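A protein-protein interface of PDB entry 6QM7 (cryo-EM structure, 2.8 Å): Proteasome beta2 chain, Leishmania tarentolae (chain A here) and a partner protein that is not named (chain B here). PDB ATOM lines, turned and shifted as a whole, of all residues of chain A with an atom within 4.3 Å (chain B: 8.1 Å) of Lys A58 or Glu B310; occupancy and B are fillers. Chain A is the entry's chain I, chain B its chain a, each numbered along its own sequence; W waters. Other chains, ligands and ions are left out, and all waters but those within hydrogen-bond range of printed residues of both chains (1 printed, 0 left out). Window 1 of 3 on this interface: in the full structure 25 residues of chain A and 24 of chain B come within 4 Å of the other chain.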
ATOM      1  N   THR A  47     -15.207   5.373  10.642  1.00  0.00           N
ATOM      2  CA  THR A  47     -15.557   6.800  10.440  1.00  0.00           C
ATOM      3  C   THR A  47     -16.304   7.402  11.631  1.00  0.00           C
ATOM      4  O   THR A  47     -16.475   8.628  11.645  1.00  0.00           O
ATOM      5  CB  THR A  47     -16.389   6.936   9.167  1.00  0.00           C
ATOM      6  OG1 THR A  47     -17.411   5.956   9.260  1.00  0.00           O
ATOM      7  CG2 THR A  47     -15.594   6.711   7.903  1.00  0.00           C
ATOM      8  N   ARG A  48     -16.721   6.606  12.605  1.00  0.00           N
ATOM      9  CA  ARG A  48     -17.622   7.092  13.670  1.00  0.00           C
ATOM     10  C   ARG A  48     -16.785   7.896  14.672  1.00  0.00           C
ATOM     11  O   ARG A  48     -15.894   7.315  15.292  1.00  0.00           O
ATOM     12  CB  ARG A  48     -18.380   5.905  14.274  1.00  0.00           C
ATOM     13  CG  ARG A  48     -19.015   6.169  15.631  1.00  0.00           C
ATOM     14  CD  ARG A  48     -19.568   4.904  16.228  1.00  0.00           C
ATOM     15  NE  ARG A  48     -20.713   4.457  15.452  1.00  0.00           N
ATOM     16  CZ  ARG A  48     -21.480   3.419  15.763  1.00  0.00           C
ATOM     17  NH1 ARG A  48     -21.241   2.708  16.849  1.00  0.00           N
ATOM     18  NH2 ARG A  48     -22.516   3.117  15.004  1.00  0.00           N
ATOM     19  N   VAL A  55     -23.035   9.255  18.829  1.00  0.00           N
ATOM     20  CA  VAL A  55     -22.360   9.492  17.528  1.00  0.00           C
ATOM     21  C   VAL A  55     -22.568  10.963  17.147  1.00  0.00           C
ATOM     22  O   VAL A  55     -23.712  11.351  16.846  1.00  0.00           O
ATOM     23  CB  VAL A  55     -22.882   8.523  16.460  1.00  0.00           C
ATOM     24  CG1 VAL A  55     -22.295   8.820  15.091  1.00  0.00           C
ATOM     25  CG2 VAL A  55     -22.633   7.076  16.870  1.00  0.00           C
ATOM     26  N   ASP A  57     -20.566  12.393  14.628  1.00  0.00           N
ATOM     27  CA  ASP A  57     -20.331  12.368  13.162  1.00  0.00           C
ATOM     28  C   ASP A  57     -20.233  10.912  12.719  1.00  0.00           C
ATOM     29  O   ASP A  57     -19.377  10.191  13.243  1.00  0.00           O
ATOM     30  CB  ASP A  57     -19.069  13.154  12.777  1.00  0.00           C
ATOM     31  CG  ASP A  57     -18.927  13.441  11.284  1.00  0.00           C
ATOM     32  OD1 ASP A  57     -19.776  12.958  10.496  1.00  0.00           O
ATOM     33  OD2 ASP A  57     -17.964  14.159  10.914  1.00  0.00           O
ATOM     34  N   LYS A  58     -21.088  10.513  11.785  1.00  0.00           N
ATOM     35  CA  LYS A  58     -21.120   9.141  11.236  1.00  0.00           C
ATOM     36  C   LYS A  58     -19.933   8.972  10.285  1.00  0.00           C
ATOM     37  O   LYS A  58     -19.242   7.957  10.405  1.00  0.00           O
ATOM     38  CB  LYS A  58     -22.474   8.879  10.576  1.00  0.00           C
ATOM     39  CG  LYS A  58     -23.648   8.828  11.545  1.00  0.00           C
ATOM     40  CD  LYS A  58     -24.958   8.406  10.899  1.00  0.00           C
ATOM     41  CE  LYS A  58     -25.706   9.551  10.243  1.00  0.00           C
ATOM     42  NZ  LYS A  58     -26.784  10.080  11.113  1.00  0.00           N
ATOM     43  N   ARG A  59     -19.688   9.956   9.419  1.00  0.00           N
ATOM     44  CA  ARG A  59     -18.654   9.925   8.353  1.00  0.00           C
ATOM     45  C   ARG A  59     -17.559  10.955   8.659  1.00  0.00           C
ATOM     46  O   ARG A  59     -17.466  11.954   7.918  1.00  0.00           O
ATOM     47  CB  ARG A  59     -19.300  10.239   6.998  1.00  0.00           C
ATOM     48  CG  ARG A  59     -19.898   9.037   6.287  1.00  0.00           C
ATOM     49  CD  ARG A  59     -20.890   9.469   5.219  1.00  0.00           C
ATOM     50  NE  ARG A  59     -22.212   9.711   5.792  1.00  0.00           N
ATOM     51  CZ  ARG A  59     -23.070   8.765   6.196  1.00  0.00           C
ATOM     52  NH1 ARG A  59     -22.764   7.476   6.100  1.00  0.00           N
ATOM     53  NH2 ARG A  59     -24.239   9.117   6.710  1.00  0.00           N
ATOM     54  N   CYS A  60     -16.765  10.750   9.706  1.00  0.00           N
ATOM     55  CA  CYS A  60     -15.570  11.590   9.985  1.00  0.00           C
ATOM     56  C   CYS A  60     -14.330  10.860   9.459  1.00  0.00           C
ATOM     57  O   CYS A  60     -14.325   9.620   9.486  1.00  0.00           O
ATOM     58  CB  CYS A  60     -15.463  11.960  11.458  1.00  0.00           C
ATOM     59  SG  CYS A  60     -14.218  11.026  12.377  1.00  0.00           S
ATOM     60  N   THR A 200     -19.855   2.615  10.987  1.00  0.00           N
ATOM     61  CA  THR A 200     -20.331   3.322   9.777  1.00  0.00           C
ATOM     62  C   THR A 200     -19.704   2.698   8.535  1.00  0.00           C
ATOM     63  O   THR A 200     -20.352   1.816   7.942  1.00  0.00           O
ATOM     64  CB  THR A 200     -20.154   4.840   9.895  1.00  0.00           C
ATOM     65  OG1 THR A 200     -20.903   5.289  11.037  1.00  0.00           O
ATOM     66  CG2 THR A 200     -20.585   5.547   8.626  1.00  0.00           C
ATOM     67  N   ARG A 224     -28.886   2.203   4.692  1.00  0.00           N
ATOM     68  CA  ARG A 224     -30.133   2.675   5.352  1.00  0.00           C
ATOM     69  C   ARG A 224     -31.121   1.507   5.505  1.00  0.00           C
ATOM     70  O   ARG A 224     -31.617   0.993   4.476  1.00  0.00           O
ATOM     71  CB  ARG A 224     -30.717   3.869   4.589  1.00  0.00           C
ATOM     72  CG  ARG A 224     -31.702   4.699   5.403  1.00  0.00           C
ATOM     73  CD  ARG A 224     -31.087   5.506   6.544  1.00  0.00           C
ATOM     74  NE  ARG A 224     -32.084   5.851   7.556  1.00  0.00           N
ATOM     75  CZ  ARG A 224     -32.017   6.876   8.411  1.00  0.00           C
ATOM     76  NH1 ARG A 224     -33.006   7.074   9.268  1.00  0.00           N
ATOM     77  NH2 ARG A 224     -30.988   7.711   8.406  1.00  0.00           N
ATOM     78  N   ALA B 267     -30.806   5.247  25.052  1.00  0.00           N
ATOM     79  CA  ALA B 267     -31.286   6.236  24.061  1.00  0.00           C
ATOM     80  C   ALA B 267     -32.597   6.891  24.523  1.00  0.00           C
ATOM     81  O   ALA B 267     -33.296   7.474  23.683  1.00  0.00           O
ATOM     82  CB  ALA B 267     -31.455   5.547  22.728  1.00  0.00           C
ATOM     83  N   PHE B 270     -32.799  10.609  23.890  1.00  0.00           N
ATOM     84  CA  PHE B 270     -33.021  10.948  22.457  1.00  0.00           C
ATOM     85  C   PHE B 270     -34.486  10.806  22.089  1.00  0.00           C
ATOM     86  O   PHE B 270     -35.007  11.647  21.341  1.00  0.00           O
ATOM     87  CB  PHE B 270     -32.382   9.969  21.468  1.00  0.00           C
ATOM     88  CG  PHE B 270     -30.890   9.864  21.514  1.00  0.00           C
ATOM     89  CD1 PHE B 270     -30.250   8.993  20.663  1.00  0.00           C
ATOM     90  CD2 PHE B 270     -30.130  10.605  22.407  1.00  0.00           C
ATOM     91  CE1 PHE B 270     -28.869   8.871  20.700  1.00  0.00           C
ATOM     92  CE2 PHE B 270     -28.749  10.484  22.441  1.00  0.00           C
ATOM     93  CZ  PHE B 270     -28.119   9.611  21.588  1.00  0.00           C
ATOM     94  N   ASN B 303     -39.354   4.669  13.425  1.00  0.00           N
ATOM     95  CA  ASN B 303     -38.551   5.867  13.084  1.00  0.00           C
ATOM     96  C   ASN B 303     -37.681   6.233  14.290  1.00  0.00           C
ATOM     97  O   ASN B 303     -36.483   6.455  14.088  1.00  0.00           O
ATOM     98  CB  ASN B 303     -39.411   7.050  12.625  1.00  0.00           C
ATOM     99  CG  ASN B 303     -38.575   8.294  12.401  1.00  0.00           C
ATOM    100  OD1 ASN B 303     -37.710   8.315  11.523  1.00  0.00           O
ATOM    101  ND2 ASN B 303     -38.786   9.322  13.214  1.00  0.00           N
ATOM    102  N   ALA B 304     -38.275   6.327  15.481  1.00  0.00           N
ATOM    103  CA  ALA B 304     -37.612   6.763  16.733  1.00  0.00           C
ATOM    104  C   ALA B 304     -36.423   5.855  17.041  1.00  0.00           C
ATOM    105  O   ALA B 304     -35.373   6.399  17.424  1.00  0.00           O
ATOM    106  CB  ALA B 304     -38.582   6.769  17.895  1.00  0.00           C
ATOM    107  N   PHE B 305     -36.594   4.542  16.879  1.00  0.00           N
ATOM    108  CA  PHE B 305     -35.558   3.504  17.119  1.00  0.00           C
ATOM    109  C   PHE B 305     -34.470   3.571  16.051  1.00  0.00           C
ATOM    110  O   PHE B 305     -33.279   3.536  16.410  1.00  0.00           O
ATOM    111  CB  PHE B 305     -36.160   2.103  17.176  1.00  0.00           C
ATOM    112  CG  PHE B 305     -36.421   1.714  18.598  1.00  0.00           C
ATOM    113  CD1 PHE B 305     -37.647   1.961  19.185  1.00  0.00           C
ATOM    114  CD2 PHE B 305     -35.397   1.209  19.380  1.00  0.00           C
ATOM    115  CE1 PHE B 305     -37.862   1.653  20.517  1.00  0.00           C
ATOM    116  CE2 PHE B 305     -35.616   0.904  20.714  1.00  0.00           C
ATOM    117  CZ  PHE B 305     -36.847   1.127  21.281  1.00  0.00           C
ATOM    118  N   THR B 306     -34.856   3.671  14.785  1.00  0.00           N
ATOM    119  CA  THR B 306     -33.895   3.864  13.673  1.00  0.00           C
ATOM    120  C   THR B 306     -32.968   5.045  13.985  1.00  0.00           C
ATOM    121  O   THR B 306     -31.766   4.906  13.759  1.00  0.00           O
ATOM    122  CB  THR B 306     -34.615   4.007  12.334  1.00  0.00           C
ATOM    123  OG1 THR B 306     -35.111   2.717  11.983  1.00  0.00           O
ATOM    124  CG2 THR B 306     -33.686   4.530  11.263  1.00  0.00           C
ATOM    125  N   GLY B 307     -33.505   6.148  14.491  1.00  0.00           N
ATOM    126  CA  GLY B 307     -32.722   7.325  14.904  1.00  0.00           C
ATOM    127  C   GLY B 307     -31.807   7.020  16.079  1.00  0.00           C
ATOM    128  O   GLY B 307     -30.621   7.396  16.010  1.00  0.00           O
ATOM    129  N   ALA B 308     -32.343   6.397  17.132  1.00  0.00           N
ATOM    130  CA  ALA B 308     -31.607   5.967  18.345  1.00  0.00           C
ATOM    131  C   ALA B 308     -30.437   5.060  17.959  1.00  0.00           C
ATOM    132  O   ALA B 308     -29.348   5.261  18.492  1.00  0.00           O
ATOM    133  CB  ALA B 308     -32.532   5.247  19.305  1.00  0.00           C
ATOM    134  N   ALA B 309     -30.684   4.088  17.085  1.00  0.00           N
ATOM    135  CA  ALA B 309     -29.703   3.083  16.617  1.00  0.00           C
ATOM    136  C   ALA B 309     -28.541   3.786  15.912  1.00  0.00           C
ATOM    137  O   ALA B 309     -27.373   3.352  16.082  1.00  0.00           O
ATOM    138  CB  ALA B 309     -30.381   2.098  15.695  1.00  0.00           C
ATOM    139  N   GLU B 310     -28.866   4.843  15.172  1.00  0.00           N
ATOM    140  CA  GLU B 310     -27.908   5.643  14.373  1.00  0.00           C
ATOM    141  C   GLU B 310     -26.925   6.382  15.292  1.00  0.00           C
ATOM    142  O   GLU B 310     -25.743   6.461  14.922  1.00  0.00           O
ATOM    143  CB  GLU B 310     -28.662   6.640  13.489  1.00  0.00           C
ATOM    144  CG  GLU B 310     -28.179   6.691  12.047  1.00  0.00           C
ATOM    145  CD  GLU B 310     -28.875   5.750  11.076  1.00  0.00           C
ATOM    146  OE1 GLU B 310     -29.792   5.016  11.507  1.00  0.00           O
ATOM    147  OE2 GLU B 310     -28.489   5.750   9.881  1.00  0.00           O
ATOM    148  N   ARG B 311     -27.393   6.895  16.430  1.00  0.00           N
ATOM    149  CA  ARG B 311     -26.667   7.889  17.264  1.00  0.00           C
ATOM    150  C   ARG B 311     -26.250   7.315  18.615  1.00  0.00           C
ATOM    151  O   ARG B 311     -25.210   7.755  19.110  1.00  0.00           O
ATOM    152  CB  ARG B 311     -27.518   9.138  17.494  1.00  0.00           C
ATOM    153  CG  ARG B 311     -27.797   9.913  16.219  1.00  0.00           C
ATOM    154  CD  ARG B 311     -26.578  10.657  15.727  1.00  0.00           C
ATOM    155  NE  ARG B 311     -26.873  11.332  14.475  1.00  0.00           N
ATOM    156  CZ  ARG B 311     -26.072  12.197  13.865  1.00  0.00           C
ATOM    157  NH1 ARG B 311     -24.897  12.515  14.383  1.00  0.00           N
ATOM    158  NH2 ARG B 311     -26.467  12.755  12.735  1.00  0.00           N
ATOM    159  N   ASP B 312     -27.040   6.432  19.220  1.00  0.00           N
ATOM    160  CA  ASP B 312     -26.663   5.752  20.486  1.00  0.00           C
ATOM    161  C   ASP B 312     -25.833   4.527  20.127  1.00  0.00           C
ATOM    162  O   ASP B 312     -26.283   3.705  19.283  1.00  0.00           O
ATOM    163  CB  ASP B 312     -27.873   5.358  21.331  1.00  0.00           C
ATOM    164  CG  ASP B 312     -27.517   4.761  22.687  1.00  0.00           C
ATOM    165  OD1 ASP B 312     -26.510   5.211  23.312  1.00  0.00           O
ATOM    166  OD2 ASP B 312     -28.246   3.842  23.108  1.00  0.00           O
ATOM    167  N   ILE B 313     -24.659   4.420  20.733  1.00  0.00           N
ATOM    168  CA  ILE B 313     -23.691   3.342  20.404  1.00  0.00           C
ATOM    169  C   ILE B 313     -24.147   2.024  21.037  1.00  0.00           C
ATOM    170  O   ILE B 313     -23.627   0.996  20.601  1.00  0.00           O
ATOM    171  CB  ILE B 313     -22.254   3.741  20.798  1.00  0.00           C
ATOM    172  CG1 ILE B 313     -22.073   3.911  22.307  1.00  0.00           C
ATOM    173  CG2 ILE B 313     -21.799   4.983  20.043  1.00  0.00           C
ATOM    174  CD1 ILE B 313     -20.640   4.156  22.687  1.00  0.00           C
ATOM    175  N   THR B 315     -27.550   1.041  21.506  1.00  0.00           N
ATOM    176  CA  THR B 315     -28.836   0.605  20.906  1.00  0.00           C
ATOM    177  C   THR B 315     -28.541   0.157  19.478  1.00  0.00           C
ATOM    178  O   THR B 315     -27.709   0.828  18.802  1.00  0.00           O
ATOM    179  CB  THR B 315     -29.871   1.734  20.962  1.00  0.00           C
ATOM    180  OG1 THR B 315     -30.005   2.066  22.345  1.00  0.00           O
ATOM    181  CG2 THR B 315     -31.215   1.365  20.364  1.00  0.00           C
ATOM    182  N   GLY B 316     -29.171  -0.929  19.043  1.00  0.00           N
ATOM    183  CA  GLY B 316     -28.972  -1.445  17.683  1.00  0.00           C
ATOM    184  C   GLY B 316     -29.533  -2.834  17.494  1.00  0.00           C
ATOM    185  O   GLY B 316     -30.192  -3.350  18.417  1.00  0.00           O
ATOM    186  N   LEU B 336     -32.428  -2.864  12.642  1.00  0.00           N
ATOM    187  CA  LEU B 336     -31.693  -1.594  12.826  1.00  0.00           C
ATOM    188  C   LEU B 336     -30.294  -1.753  12.240  1.00  0.00           C
ATOM    189  O   LEU B 336     -29.955  -2.869  11.816  1.00  0.00           O
ATOM    190  CB  LEU B 336     -31.595  -1.290  14.319  1.00  0.00           C
ATOM    191  CG  LEU B 336     -32.910  -1.152  15.082  1.00  0.00           C
ATOM    192  CD1 LEU B 336     -32.626  -0.955  16.569  1.00  0.00           C
ATOM    193  CD2 LEU B 336     -33.759  -0.014  14.527  1.00  0.00           C
ATOM    194  N   ARG B 337     -29.516  -0.670  12.236  1.00  0.00           N
ATOM    195  CA  ARG B 337     -28.056  -0.690  11.950  1.00  0.00           C
ATOM    196  C   ARG B 337     -27.390  -1.763  12.816  1.00  0.00           C
ATOM    197  O   ARG B 337     -27.512  -1.686  14.062  1.00  0.00           O
ATOM    198  CB  ARG B 337     -27.421   0.674  12.223  1.00  0.00           C
ATOM    199  CG  ARG B 337     -26.973   1.404  10.969  1.00  0.00           C
ATOM    200  CD  ARG B 337     -26.922   2.891  11.233  1.00  0.00           C
ATOM    201  NE  ARG B 337     -26.096   3.616  10.278  1.00  0.00           N
ATOM    202  CZ  ARG B 337     -24.785   3.846  10.393  1.00  0.00           C
ATOM    203  NH1 ARG B 337     -24.164   4.539   9.451  1.00  0.00           N
ATOM    204  NH2 ARG B 337     -24.095   3.400  11.434  1.00  0.00           N
ATOM    205  N   ASP B 339     -24.260  -2.349  13.223  1.00  0.00           N
ATOM    206  CA  ASP B 339     -23.014  -1.814  13.840  1.00  0.00           C
ATOM    207  C   ASP B 339     -23.331  -1.071  15.150  1.00  0.00           C
ATOM    208  O   ASP B 339     -22.509  -1.137  16.079  1.00  0.00           O
ATOM    209  CB  ASP B 339     -22.236  -0.929  12.858  1.00  0.00           C
ATOM    210  CG  ASP B 339     -22.661   0.529  12.784  1.00  0.00           C
ATOM    211  OD1 ASP B 339     -21.882   1.376  13.236  1.00  0.00           O
ATOM    212  OD2 ASP B 339     -23.740   0.811  12.245  1.00  0.00           O
ATOM    213  OXT ASP B 339     -24.370  -0.402  15.334  1.00  0.00           O
HETATM  214  O   HOH W   1     -22.685   0.969  18.120  1.00  0.00           O
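Water W1 lies within hydrogen-bond range of the guanidinium group of Arg A48, the backbone carbonyl oxygen of Ile B313 and the chain-end carboxylate of Asp B339.
Of chain B, only Glu B310 (3.8 Å) and Arg B311 (3.1 Å) come within 4 Å of Lys A58.
Of the printed residues of chain A, Glu B310 touches Val A55 (3.7 Å), Lys A58 (3.8 Å) and Arg A224 (3.5 Å).
Printed residues of chain B within 4 Å of Val A55: Glu B310 (3.7 Å), Arg B311 (2.7 Å) and Ile B313 (3.9 Å).
Printed residues of chain B within 4 Å of Arg A48: Ile B313 (3.96 Å), Arg B337 (3.9 Å) and Asp B339 (2.6 Å).
Ala B308 touches none of the printed residues of chain A.
The nearest residue of chain B that does not touch Lys A58 is Arg B337 (4.2 Å).
The nearest printed residue of chain A that does not touch Asp B339 is Val A55 (6.8 Å).
Among the printed residues, pairs that only touch across the chains: Arg A224 with Thr B306 (3.3 Å), Thr A200 with Arg B337 (3.7 Å), Val A55 with Glu B310 (3.7 Å), Lys A58 with Glu B310 (3.8 Å), Val A55 with Ile B313 (3.9 Å), Arg A48 with Arg B337 (3.9 Å) and Arg A48 with Ile B313 (3.96 Å).
OD1 of Asp B339 lies within salt-bridge range of NH2 of Arg A48 (2.6 Å).
The side-chain carboxylate of Asp B339 sits at hydrogen-bond distance from the backbone NH of Thr A200 (3.3 Å).
O of Arg B311 is in hydrogen-bond range of N of Val A55 (2.7 Å).
OE2 of Glu B310 is in salt-bridge range of NH2 of Arg A224, at 3.5 Å.
The side-chain amino group (NZ) of Lys A58 sits close to the guanidinium group (NH2) of Arg B311, at 3.1 Å.
The side-chain carboxylate (OE2) of Glu B310 is in salt-bridge range of the guanidinium group (NE) of Arg B337.
The backbone carbonyl oxygen (O) of Lys A58 sits at hydrogen-bond distance from the side-chain hydroxyl (OG1) of Thr A200, 3.2 Å away.
The guanidinium group of Arg B337 is in salt-bridge range of the side-chain carboxylate of Asp B339 (2.7 Å).
The side-chain hydroxyl (OG1) of Thr A47 is in hydrogen-bond range of the backbone carbonyl oxygen (O) of Lys A58 (2.9 Å).
Hydrophobic or aromatic side chains of chain A within 4 Å of the printed part of chain B: Val A55.
Printed residues of chain B that touch a printed residue of chain A: Thr B306, Glu B310, Arg B311, Ile B313, Arg B337 and Asp B339.
Hydrophobic or aromatic side chains of chain B that line the printed part of chain A: Ile B313.
Among the printed residues, 12 pairs touch across the chains.
Among the printed residues, Asp or Glu carboxylates within 4 Å of a Lys or Arg side-chain nitrogen of the other chain: Arg A48 with Asp B339 (2.6 Å) and Arg A224 with Glu B310 (3.5 Å).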
